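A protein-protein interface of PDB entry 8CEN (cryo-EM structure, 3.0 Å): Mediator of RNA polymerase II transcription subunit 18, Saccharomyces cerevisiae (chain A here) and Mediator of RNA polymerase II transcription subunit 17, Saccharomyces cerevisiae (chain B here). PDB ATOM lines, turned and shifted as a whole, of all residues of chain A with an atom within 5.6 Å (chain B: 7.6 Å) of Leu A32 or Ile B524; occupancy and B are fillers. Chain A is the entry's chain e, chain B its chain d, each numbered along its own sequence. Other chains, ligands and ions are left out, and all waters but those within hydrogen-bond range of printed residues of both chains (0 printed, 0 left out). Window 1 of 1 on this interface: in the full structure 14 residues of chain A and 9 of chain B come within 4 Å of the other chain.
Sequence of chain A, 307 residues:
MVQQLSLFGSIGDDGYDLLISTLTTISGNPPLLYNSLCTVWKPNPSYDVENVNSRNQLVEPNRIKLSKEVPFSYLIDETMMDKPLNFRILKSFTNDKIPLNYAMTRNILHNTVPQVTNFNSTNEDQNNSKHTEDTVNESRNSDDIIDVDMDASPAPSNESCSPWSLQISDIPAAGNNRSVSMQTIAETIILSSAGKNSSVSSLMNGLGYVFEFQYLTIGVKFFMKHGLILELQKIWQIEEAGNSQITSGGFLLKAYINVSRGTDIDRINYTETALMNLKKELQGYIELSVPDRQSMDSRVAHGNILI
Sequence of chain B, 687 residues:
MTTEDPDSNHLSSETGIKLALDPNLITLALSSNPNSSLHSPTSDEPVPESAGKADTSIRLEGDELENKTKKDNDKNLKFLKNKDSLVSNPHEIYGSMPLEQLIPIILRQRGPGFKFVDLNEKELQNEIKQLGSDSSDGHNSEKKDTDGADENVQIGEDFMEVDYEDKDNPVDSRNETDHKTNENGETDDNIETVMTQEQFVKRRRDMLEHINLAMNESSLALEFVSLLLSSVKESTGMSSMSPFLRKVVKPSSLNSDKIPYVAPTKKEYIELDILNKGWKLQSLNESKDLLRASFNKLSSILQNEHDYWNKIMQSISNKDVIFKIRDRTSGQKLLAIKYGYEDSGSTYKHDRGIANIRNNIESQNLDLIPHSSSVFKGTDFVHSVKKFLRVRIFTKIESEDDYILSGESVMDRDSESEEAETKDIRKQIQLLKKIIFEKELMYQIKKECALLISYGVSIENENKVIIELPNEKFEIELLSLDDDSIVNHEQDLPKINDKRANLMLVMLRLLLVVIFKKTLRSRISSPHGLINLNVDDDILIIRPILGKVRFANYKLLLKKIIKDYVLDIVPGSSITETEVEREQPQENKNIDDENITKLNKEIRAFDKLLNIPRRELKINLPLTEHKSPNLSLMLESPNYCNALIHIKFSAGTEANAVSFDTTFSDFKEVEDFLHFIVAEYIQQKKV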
ATOM      1  N   ASN A  29      33.724  -9.509  22.680  1.00  0.00           N
ATOM      2  CA  ASN A  29      32.859  -9.958  23.751  1.00  0.00           C
ATOM      3  C   ASN A  29      33.367  -9.445  25.093  1.00  0.00           C
ATOM      4  O   ASN A  29      34.574  -9.498  25.357  1.00  0.00           O
ATOM      5  CB  ASN A  29      32.790 -11.492  23.787  1.00  0.00           C
ATOM      6  CG  ASN A  29      32.064 -12.072  22.591  1.00  0.00           C
ATOM      7  OD1 ASN A  29      31.041 -11.544  22.156  1.00  0.00           O
ATOM      8  ND2 ASN A  29      32.592 -13.164  22.052  1.00  0.00           N
ATOM      9  N   PRO A  30      32.482  -8.926  25.948  1.00  0.00           N
ATOM     10  CA  PRO A  30      32.917  -8.508  27.279  1.00  0.00           C
ATOM     11  C   PRO A  30      33.306  -9.707  28.123  1.00  0.00           C
ATOM     12  O   PRO A  30      32.814 -10.828  27.899  1.00  0.00           O
ATOM     13  CB  PRO A  30      31.676  -7.797  27.852  1.00  0.00           C
ATOM     14  CG  PRO A  30      30.823  -7.479  26.668  1.00  0.00           C
ATOM     15  CD  PRO A  30      31.080  -8.569  25.682  1.00  0.00           C
ATOM     16  N   PRO A  31      34.203  -9.529  29.094  1.00  0.00           N
ATOM     17  CA  PRO A  31      34.559 -10.639  29.986  1.00  0.00           C
ATOM     18  C   PRO A  31      33.397 -11.049  30.877  1.00  0.00           C
ATOM     19  O   PRO A  31      32.514 -10.251  31.198  1.00  0.00           O
ATOM     20  CB  PRO A  31      35.720 -10.072  30.810  1.00  0.00           C
ATOM     21  CG  PRO A  31      35.537  -8.599  30.752  1.00  0.00           C
ATOM     22  CD  PRO A  31      34.972  -8.310  29.396  1.00  0.00           C
ATOM     23  N   LEU A  32      33.407 -12.321  31.273  1.00  0.00           N
ATOM     24  CA  LEU A  32      32.299 -12.934  31.998  1.00  0.00           C
ATOM     25  C   LEU A  32      32.790 -13.454  33.341  1.00  0.00           C
ATOM     26  O   LEU A  32      33.470 -14.484  33.397  1.00  0.00           O
ATOM     27  CB  LEU A  32      31.680 -14.059  31.178  1.00  0.00           C
ATOM     28  CG  LEU A  32      31.004 -13.556  29.912  1.00  0.00           C
ATOM     29  CD1 LEU A  32      30.532 -14.722  29.070  1.00  0.00           C
ATOM     30  CD2 LEU A  32      29.858 -12.643  30.306  1.00  0.00           C
ATOM     31  N   LEU A  33      32.414 -12.763  34.415  1.00  0.00           N
ATOM     32  CA  LEU A  33      32.792 -13.180  35.759  1.00  0.00           C
ATOM     33  C   LEU A  33      32.131 -14.508  36.107  1.00  0.00           C
ATOM     34  O   LEU A  33      30.926 -14.688  35.909  1.00  0.00           O
ATOM     35  CB  LEU A  33      32.399 -12.107  36.773  1.00  0.00           C
ATOM     36  CG  LEU A  33      32.976 -12.203  38.183  1.00  0.00           C
ATOM     37  CD1 LEU A  33      34.457 -11.865  38.192  1.00  0.00           C
ATOM     38  CD2 LEU A  33      32.205 -11.281  39.112  1.00  0.00           C
ATOM     39  N   TYR A  34      32.930 -15.441  36.621  1.00  0.00           N
ATOM     40  CA  TYR A  34      32.462 -16.779  36.941  1.00  0.00           C
ATOM     41  C   TYR A  34      33.206 -17.290  38.164  1.00  0.00           C
ATOM     42  O   TYR A  34      34.263 -16.776  38.535  1.00  0.00           O
ATOM     43  CB  TYR A  34      32.652 -17.743  35.756  1.00  0.00           C
ATOM     44  CG  TYR A  34      34.074 -18.241  35.567  1.00  0.00           C
ATOM     45  CD1 TYR A  34      35.019 -17.463  34.914  1.00  0.00           C
ATOM     46  CD2 TYR A  34      34.460 -19.500  36.017  1.00  0.00           C
ATOM     47  CE1 TYR A  34      36.316 -17.913  34.734  1.00  0.00           C
ATOM     48  CE2 TYR A  34      35.756 -19.956  35.843  1.00  0.00           C
ATOM     49  CZ  TYR A  34      36.677 -19.159  35.200  1.00  0.00           C
ATOM     50  OH  TYR A  34      37.964 -19.610  35.022  1.00  0.00           O
ATOM     51  N   GLY A 219      37.140 -15.888  38.289  1.00  0.00           N
ATOM     52  CA  GLY A 219      37.796 -15.291  37.151  1.00  0.00           C
ATOM     53  C   GLY A 219      36.812 -14.768  36.132  1.00  0.00           C
ATOM     54  O   GLY A 219      35.603 -14.729  36.366  1.00  0.00           O
ATOM     55  N   VAL A 220      37.361 -14.351  34.994  1.00  0.00           N
ATOM     56  CA  VAL A 220      36.587 -13.862  33.860  1.00  0.00           C
ATOM     57  C   VAL A 220      36.987 -14.647  32.618  1.00  0.00           C
ATOM     58  O   VAL A 220      38.158 -15.005  32.447  1.00  0.00           O
ATOM     59  CB  VAL A 220      36.772 -12.343  33.649  1.00  0.00           C
ATOM     60  CG1 VAL A 220      36.153 -11.571  34.801  1.00  0.00           C
ATOM     61  CG2 VAL A 220      38.244 -11.989  33.536  1.00  0.00           C
ATOM     62  N   LYS A 221      36.013 -14.939  31.759  1.00  0.00           N
ATOM     63  CA  LYS A 221      36.282 -15.701  30.550  1.00  0.00           C
ATOM     64  C   LYS A 221      35.743 -14.983  29.320  1.00  0.00           C
ATOM     65  O   LYS A 221      34.834 -14.154  29.400  1.00  0.00           O
ATOM     66  CB  LYS A 221      35.695 -17.118  30.607  1.00  0.00           C
ATOM     67  CG  LYS A 221      34.185 -17.186  30.670  1.00  0.00           C
ATOM     68  CD  LYS A 221      33.739 -18.636  30.683  1.00  0.00           C
ATOM     69  CE  LYS A 221      34.035 -19.294  32.013  1.00  0.00           C
ATOM     70  NZ  LYS A 221      33.482 -20.672  32.068  1.00  0.00           N
ATOM     71  N   PHE A 222      36.334 -15.322  28.176  1.00  0.00           N
ATOM     72  CA  PHE A 222      35.944 -14.795  26.876  1.00  0.00           C
ATOM     73  C   PHE A 222      35.550 -15.951  25.968  1.00  0.00           C
ATOM     74  O   PHE A 222      36.252 -16.966  25.911  1.00  0.00           O
ATOM     75  CB  PHE A 222      37.082 -13.999  26.228  1.00  0.00           C
ATOM     76  CG  PHE A 222      37.521 -12.797  27.016  1.00  0.00           C
ATOM     77  CD1 PHE A 222      38.466 -12.912  28.023  1.00  0.00           C
ATOM     78  CD2 PHE A 222      36.997 -11.546  26.734  1.00  0.00           C
ATOM     79  CE1 PHE A 222      38.870 -11.805  28.742  1.00  0.00           C
ATOM     80  CE2 PHE A 222      37.399 -10.435  27.448  1.00  0.00           C
ATOM     81  CZ  PHE A 222      38.338 -10.564  28.451  1.00  0.00           C
ATOM     82  N   PHE A 223      34.431 -15.797  25.265  1.00  0.00           N
ATOM     83  CA  PHE A 223      34.009 -16.748  24.238  1.00  0.00           C
ATOM     84  C   PHE A 223      34.333 -16.122  22.886  1.00  0.00           C
ATOM     85  O   PHE A 223      33.507 -15.437  22.284  1.00  0.00           O
ATOM     86  CB  PHE A 223      32.526 -17.077  24.365  1.00  0.00           C
ATOM     87  CG  PHE A 223      32.187 -17.910  25.566  1.00  0.00           C
ATOM     88  CD1 PHE A 223      33.054 -18.888  26.023  1.00  0.00           C
ATOM     89  CD2 PHE A 223      30.994 -17.719  26.234  1.00  0.00           C
ATOM     90  CE1 PHE A 223      32.731 -19.654  27.129  1.00  0.00           C
ATOM     91  CE2 PHE A 223      30.666 -18.480  27.340  1.00  0.00           C
ATOM     92  CZ  PHE A 223      31.537 -19.449  27.788  1.00  0.00           C
ATOM     93  N   LYS B 517      20.394  -8.110  19.806  1.00  0.00           N
ATOM     94  CA  LYS B 517      20.687  -8.377  21.209  1.00  0.00           C
ATOM     95  C   LYS B 517      20.552  -9.854  21.546  1.00  0.00           C
ATOM     96  O   LYS B 517      21.301 -10.361  22.383  1.00  0.00           O
ATOM     97  CB  LYS B 517      19.774  -7.539  22.097  1.00  0.00           C
ATOM     98  CG  LYS B 517      20.108  -6.078  22.018  1.00  0.00           C
ATOM     99  CD  LYS B 517      19.258  -5.226  22.915  1.00  0.00           C
ATOM    100  CE  LYS B 517      19.664  -3.783  22.739  1.00  0.00           C
ATOM    101  NZ  LYS B 517      21.010  -3.513  23.313  1.00  0.00           N
ATOM    102  N   LYS B 518      19.620 -10.561  20.906  1.00  0.00           N
ATOM    103  CA  LYS B 518      19.509 -12.000  21.123  1.00  0.00           C
ATOM    104  C   LYS B 518      20.701 -12.742  20.533  1.00  0.00           C
ATOM    105  O   LYS B 518      21.186 -13.715  21.123  1.00  0.00           O
ATOM    106  CB  LYS B 518      18.202 -12.523  20.530  1.00  0.00           C
ATOM    107  CG  LYS B 518      16.997 -12.343  21.436  1.00  0.00           C
ATOM    108  CD  LYS B 518      15.758 -12.976  20.831  1.00  0.00           C
ATOM    109  CE  LYS B 518      14.636 -13.066  21.849  1.00  0.00           C
ATOM    110  NZ  LYS B 518      14.232 -11.721  22.339  1.00  0.00           N
ATOM    111  N   THR B 519      21.187 -12.296  19.371  1.00  0.00           N
ATOM    112  CA  THR B 519      22.396 -12.882  18.796  1.00  0.00           C
ATOM    113  C   THR B 519      23.610 -12.620  19.683  1.00  0.00           C
ATOM    114  O   THR B 519      24.445 -13.512  19.893  1.00  0.00           O
ATOM    115  CB  THR B 519      22.626 -12.328  17.390  1.00  0.00           C
ATOM    116  OG1 THR B 519      21.450 -12.535  16.597  1.00  0.00           O
ATOM    117  CG2 THR B 519      23.806 -13.018  16.722  1.00  0.00           C
ATOM    118  N   LEU B 520      23.710 -11.401  20.226  1.00  0.00           N
ATOM    119  CA  LEU B 520      24.772 -11.093  21.178  1.00  0.00           C
ATOM    120  C   LEU B 520      24.657 -11.953  22.430  1.00  0.00           C
ATOM    121  O   LEU B 520      25.664 -12.462  22.928  1.00  0.00           O
ATOM    122  CB  LEU B 520      24.740  -9.611  21.547  1.00  0.00           C
ATOM    123  CG  LEU B 520      25.397  -8.639  20.569  1.00  0.00           C
ATOM    124  CD1 LEU B 520      25.279  -7.213  21.081  1.00  0.00           C
ATOM    125  CD2 LEU B 520      26.851  -9.013  20.338  1.00  0.00           C
ATOM    126  N   ARG B 521      23.436 -12.137  22.939  1.00  0.00           N
ATOM    127  CA  ARG B 521      23.224 -12.962  24.123  1.00  0.00           C
ATOM    128  C   ARG B 521      23.604 -14.412  23.861  1.00  0.00           C
ATOM    129  O   ARG B 521      24.145 -15.085  24.742  1.00  0.00           O
ATOM    130  CB  ARG B 521      21.767 -12.860  24.576  1.00  0.00           C
ATOM    131  CG  ARG B 521      21.430 -13.699  25.797  1.00  0.00           C
ATOM    132  CD  ARG B 521      20.151 -13.233  26.463  1.00  0.00           C
ATOM    133  NE  ARG B 521      18.968 -13.800  25.829  1.00  0.00           N
ATOM    134  CZ  ARG B 521      17.723 -13.566  26.223  1.00  0.00           C
ATOM    135  NH1 ARG B 521      17.462 -12.786  27.258  1.00  0.00           N
ATOM    136  NH2 ARG B 521      16.717 -14.133  25.563  1.00  0.00           N
ATOM    137  N   SER B 522      23.328 -14.909  22.653  1.00  0.00           N
ATOM    138  CA  SER B 522      23.765 -16.251  22.280  1.00  0.00           C
ATOM    139  C   SER B 522      25.287 -16.349  22.258  1.00  0.00           C
ATOM    140  O   SER B 522      25.867 -17.307  22.784  1.00  0.00           O
ATOM    141  CB  SER B 522      23.180 -16.632  20.920  1.00  0.00           C
ATOM    142  OG  SER B 522      23.646 -17.904  20.506  1.00  0.00           O
ATOM    143  N   ARG B 523      25.952 -15.351  21.665  1.00  0.00           N
ATOM    144  CA  ARG B 523      27.412 -15.373  21.586  1.00  0.00           C
ATOM    145  C   ARG B 523      28.081 -15.178  22.943  1.00  0.00           C
ATOM    146  O   ARG B 523      29.237 -15.580  23.112  1.00  0.00           O
ATOM    147  CB  ARG B 523      27.904 -14.309  20.603  1.00  0.00           C
ATOM    148  CG  ARG B 523      27.537 -14.594  19.155  1.00  0.00           C
ATOM    149  CD  ARG B 523      28.603 -14.087  18.197  1.00  0.00           C
ATOM    150  NE  ARG B 523      28.593 -12.635  18.081  1.00  0.00           N
ATOM    151  CZ  ARG B 523      28.225 -11.972  16.993  1.00  0.00           C
ATOM    152  NH1 ARG B 523      27.826 -12.604  15.900  1.00  0.00           N
ATOM    153  NH2 ARG B 523      28.257 -10.643  17.000  1.00  0.00           N
ATOM    154  N   ILE B 524      27.389 -14.571  23.903  1.00  0.00           N
ATOM    155  CA  ILE B 524      27.906 -14.445  25.267  1.00  0.00           C
ATOM    156  C   ILE B 524      27.596 -15.680  26.111  1.00  0.00           C
ATOM    157  O   ILE B 524      28.429 -16.118  26.906  1.00  0.00           O
ATOM    158  CB  ILE B 524      27.368 -13.148  25.916  1.00  0.00           C
ATOM    159  CG1 ILE B 524      27.800 -11.919  25.114  1.00  0.00           C
ATOM    160  CG2 ILE B 524      27.783 -13.013  27.356  1.00  0.00           C
ATOM    161  CD1 ILE B 524      29.292 -11.749  25.032  1.00  0.00           C
ATOM    162  N   SER B 525      26.416 -16.280  25.958  1.00  0.00           N
ATOM    163  CA  SER B 525      26.054 -17.425  26.782  1.00  0.00           C
ATOM    164  C   SER B 525      26.612 -18.741  26.257  1.00  0.00           C
ATOM    165  O   SER B 525      26.622 -19.730  26.998  1.00  0.00           O
ATOM    166  CB  SER B 525      24.532 -17.527  26.900  1.00  0.00           C
ATOM    167  OG  SER B 525      23.998 -16.413  27.593  1.00  0.00           O
ATOM    168  N   SER B 526      27.079 -18.784  25.012  1.00  0.00           N
ATOM    169  CA  SER B 526      27.606 -20.027  24.473  1.00  0.00           C
ATOM    170  C   SER B 526      28.999 -19.806  23.904  1.00  0.00           C
ATOM    171  O   SER B 526      29.308 -18.717  23.409  1.00  0.00           O
ATOM    172  CB  SER B 526      26.684 -20.587  23.380  1.00  0.00           C
ATOM    173  OG  SER B 526      26.625 -19.715  22.267  1.00  0.00           O
ATOM    174  N   PRO B 527      29.867 -20.823  23.970  1.00  0.00           N
ATOM    175  CA  PRO B 527      31.213 -20.655  23.397  1.00  0.00           C
ATOM    176  C   PRO B 527      31.219 -20.622  21.880  1.00  0.00           C
ATOM    177  O   PRO B 527      31.971 -19.839  21.289  1.00  0.00           O
ATOM    178  CB  PRO B 527      31.979 -21.868  23.945  1.00  0.00           C
ATOM    179  CG  PRO B 527      30.923 -22.871  24.267  1.00  0.00           C
ATOM    180  CD  PRO B 527      29.742 -22.077  24.732  1.00  0.00           C
ATOM    181  N   GLY B 529      28.609 -19.772  19.873  1.00  0.00           N
ATOM    182  CA  GLY B 529      27.907 -18.580  19.454  1.00  0.00           C
ATOM    183  C   GLY B 529      26.986 -18.833  18.272  1.00  0.00           C
ATOM    184  O   GLY B 529      27.072 -19.840  17.572  1.00  0.00           O
ATOM    185  N   LEU B 530      26.081 -17.884  18.054  1.00  0.00           N
ATOM    186  CA  LEU B 530      25.172 -17.959  16.922  1.00  0.00           C
ATOM    187  C   LEU B 530      25.876 -17.428  15.679  1.00  0.00           C
ATOM    188  O   LEU B 530      26.394 -16.307  15.680  1.00  0.00           O
ATOM    189  CB  LEU B 530      23.892 -17.169  17.213  1.00  0.00           C
ATOM    190  CG  LEU B 530      22.678 -17.266  16.278  1.00  0.00           C
ATOM    191  CD1 LEU B 530      21.402 -17.070  17.078  1.00  0.00           C
ATOM    192  CD2 LEU B 530      22.727 -16.251  15.141  1.00  0.00           C
ATOM    193  N   ILE B 591      23.810 -17.201  36.531  1.00  0.00           N
ATOM    194  CA  ILE B 591      24.725 -16.721  35.502  1.00  0.00           C
ATOM    195  C   ILE B 591      25.090 -15.268  35.775  1.00  0.00           C
ATOM    196  O   ILE B 591      25.282 -14.486  34.839  1.00  0.00           O
ATOM    197  CB  ILE B 591      24.117 -16.885  34.097  1.00  0.00           C
ATOM    198  CG1 ILE B 591      22.669 -16.386  34.079  1.00  0.00           C
ATOM    199  CG2 ILE B 591      24.196 -18.336  33.645  1.00  0.00           C
ATOM    200  CD1 ILE B 591      22.023 -16.436  32.710  1.00  0.00           C
ATOM    201  N   ASP B 592      25.175 -14.899  37.055  1.00  0.00           N
ATOM    202  CA  ASP B 592      25.311 -13.506  37.476  1.00  0.00           C
ATOM    203  C   ASP B 592      26.581 -12.826  36.969  1.00  0.00           C
ATOM    204  O   ASP B 592      27.692 -13.154  37.396  1.00  0.00           O
ATOM    205  CB  ASP B 592      25.254 -13.417  39.003  1.00  0.00           C
ATOM    206  CG  ASP B 592      23.838 -13.518  39.540  1.00  0.00           C
ATOM    207  OD1 ASP B 592      22.899 -13.641  38.726  1.00  0.00           O
ATOM    208  OD2 ASP B 592      23.665 -13.471  40.775  1.00  0.00           O
ATOM    209  N   ASP B 593      26.403 -11.873  36.056  1.00  0.00           N
ATOM    210  CA  ASP B 593      27.447 -10.985  35.561  1.00  0.00           C
ATOM    211  C   ASP B 593      26.741  -9.768  34.981  1.00  0.00           C
ATOM    212  O   ASP B 593      25.608  -9.873  34.508  1.00  0.00           O
ATOM    213  CB  ASP B 593      28.340 -11.678  34.516  1.00  0.00           C
ATOM    214  CG  ASP B 593      29.485 -10.794  34.015  1.00  0.00           C
ATOM    215  OD1 ASP B 593      29.246  -9.717  33.425  1.00  0.00           O
ATOM    216  OD2 ASP B 593      30.648 -11.179  34.220  1.00  0.00           O
ATOM    217  N   GLU B 594      27.429  -8.621  35.016  1.00  0.00           N
ATOM    218  CA  GLU B 594      26.794  -7.347  34.682  1.00  0.00           C
ATOM    219  C   GLU B 594      26.282  -7.328  33.247  1.00  0.00           C
ATOM    220  O   GLU B 594      25.115  -7.005  33.004  1.00  0.00           O
ATOM    221  CB  GLU B 594      27.768  -6.191  34.911  1.00  0.00           C
ATOM    222  CG  GLU B 594      27.168  -4.819  34.636  1.00  0.00           C
ATOM    223  CD  GLU B 594      28.223  -3.753  34.411  1.00  0.00           C
ATOM    224  OE1 GLU B 594      29.382  -3.969  34.821  1.00  0.00           O
ATOM    225  OE2 GLU B 594      27.893  -2.699  33.828  1.00  0.00           O
ATOM    226  N   ASN B 595      27.137  -7.693  32.288  1.00  0.00           N
ATOM    227  CA  ASN B 595      26.770  -7.604  30.876  1.00  0.00           C
ATOM    228  C   ASN B 595      25.634  -8.559  30.525  1.00  0.00           C
ATOM    229  O   ASN B 595      24.692  -8.179  29.819  1.00  0.00           O
ATOM    230  CB  ASN B 595      27.990  -7.882  29.998  1.00  0.00           C
ATOM    231  CG  ASN B 595      29.219  -7.111  30.442  1.00  0.00           C
ATOM    232  OD1 ASN B 595      29.453  -5.988  29.996  1.00  0.00           O
ATOM    233  ND2 ASN B 595      30.017  -7.715  31.315  1.00  0.00           N
ATOM    234  N   ILE B 596      25.695  -9.797  31.021  1.00  0.00           N
ATOM    235  CA  ILE B 596      24.664 -10.765  30.666  1.00  0.00           C
ATOM    236  C   ILE B 596      23.348 -10.451  31.378  1.00  0.00           C
ATOM    237  O   ILE B 596      22.273 -10.676  30.813  1.00  0.00           O
ATOM    238  CB  ILE B 596      25.161 -12.203  30.929  1.00  0.00           C
ATOM    239  CG1 ILE B 596      24.142 -13.242  30.448  1.00  0.00           C
ATOM    240  CG2 ILE B 596      25.484 -12.413  32.383  1.00  0.00           C
ATOM    241  CD1 ILE B 596      24.661 -14.663  30.462  1.00  0.00           C
ATOM    242  N   THR B 597      23.387  -9.893  32.597  1.00  0.00           N
ATOM    243  CA  THR B 597      22.128  -9.477  33.217  1.00  0.00           C
ATOM    244  C   THR B 597      21.536  -8.242  32.550  1.00  0.00           C
ATOM    245  O   THR B 597      20.308  -8.132  32.465  1.00  0.00           O
ATOM    246  CB  THR B 597      22.287  -9.240  34.721  1.00  0.00           C
ATOM    247  OG1 THR B 597      23.210  -8.168  34.962  1.00  0.00           O
ATOM    248  CG2 THR B 597      22.679 -10.520  35.459  1.00  0.00           C
ATOM    249  N   LEU B 599      21.840  -7.729  29.330  1.00  0.00           N
ATOM    250  CA  LEU B 599      21.254  -8.336  28.136  1.00  0.00           C
ATOM    251  C   LEU B 599      19.934  -9.033  28.452  1.00  0.00           C
ATOM    252  O   LEU B 599      18.960  -8.905  27.701  1.00  0.00           O
ATOM    253  CB  LEU B 599      22.241  -9.321  27.512  1.00  0.00           C
ATOM    254  CG  LEU B 599      23.394  -8.713  26.714  1.00  0.00           C
ATOM    255  CD1 LEU B 599      24.324  -9.800  26.205  1.00  0.00           C
ATOM    256  CD2 LEU B 599      22.860  -7.882  25.560  1.00  0.00           C
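N of Leu A33 lies close to OD2 of Asp B593 (2.4 Å).
Of the printed residues of chain B, Pro A30 touches Ile B524 and Asn B595. Of the printed residues of chain B, Pro A31 touches Asp B593 and Asn B595. Leu A32 touches just these residues of chain B: Ile B524 and Asp B593. Printed residues of chain B within 4 Å of Leu A33: Asp B592 (3.9 Å) and Asp B593 (2.4 Å). Of the printed residues of chain A, Arg B523 touches Phe A223 (3.8 Å). Ile B524 touches just these residues of chain A: Asn A29, Pro A30, Leu A32 and Phe A223. Of the printed residues of chain A, Asp B592 touches Leu A33 (3.9 Å). Glu B594 touches none of the printed residues of chain A. The nearest residue of chain B that does not touch Leu A32 is Ile B596 (4.8 Å). The nearest printed residue of chain A that does not touch Ile B524 is Pro A31 (6.7 Å). The nearest printed residue of chain B that does not touch Leu A33 is Ile B591 (5.7 Å).
OG of Ser B526 sits at hydrogen-bond distance from O of Ser B522, at 2.6 Å. OG of Ser B526 is in hydrogen-bond range of N of Gly B529 (3.1 Å). The backbone NH (N) of Leu A32 sits at hydrogen-bond distance from the backbone carbonyl oxygen (O) of Lys A221, at 3.0 Å. The backbone carbonyl oxygen (O) of Asp B593 lies within hydrogen-bond range of the side-chain hydroxyl (OG1) of Thr B597, 3.0 Å away. ND2 of Asn B595 sits at hydrogen-bond distance from OD1 of Asp B593, 3.0 Å away. The side-chain amide nitrogen of Asn A29 sits at hydrogen-bond distance from the backbone carbonyl oxygen of Phe A223, 2.5 Å away.
Among the printed residues, merely in contact across the chains: Asn A29 with Ile B524 (3.4 Å), Pro A30 with Ile B524 (3.7 Å), Pro A30 with Asn B595 (3.6 Å), Pro A31 with Asp B593 (3.7 Å), Pro A31 with Asn B595 (3.6 Å), Leu A32 with Ile B524 (3.3 Å), Leu A32 with Asp B593 (3.2 Å), Leu A33 with Asp B592 (3.9 Å), Phe A223 with Arg B523 (3.8 Å), Phe A223 with Ile B524 (3.1 Å), Phe A223 with Ser B526 (3.4 Å) and Phe A223 with Pro B527 (3.6 Å).
Hydrophobic or aromatic side chains of chain B that line the printed part of chain A: Ile B524 and Pro B527. Among the printed residues, no Asp or Glu carboxylate lies within 4 Å of a Lys or Arg side-chain nitrogen of the other chain.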
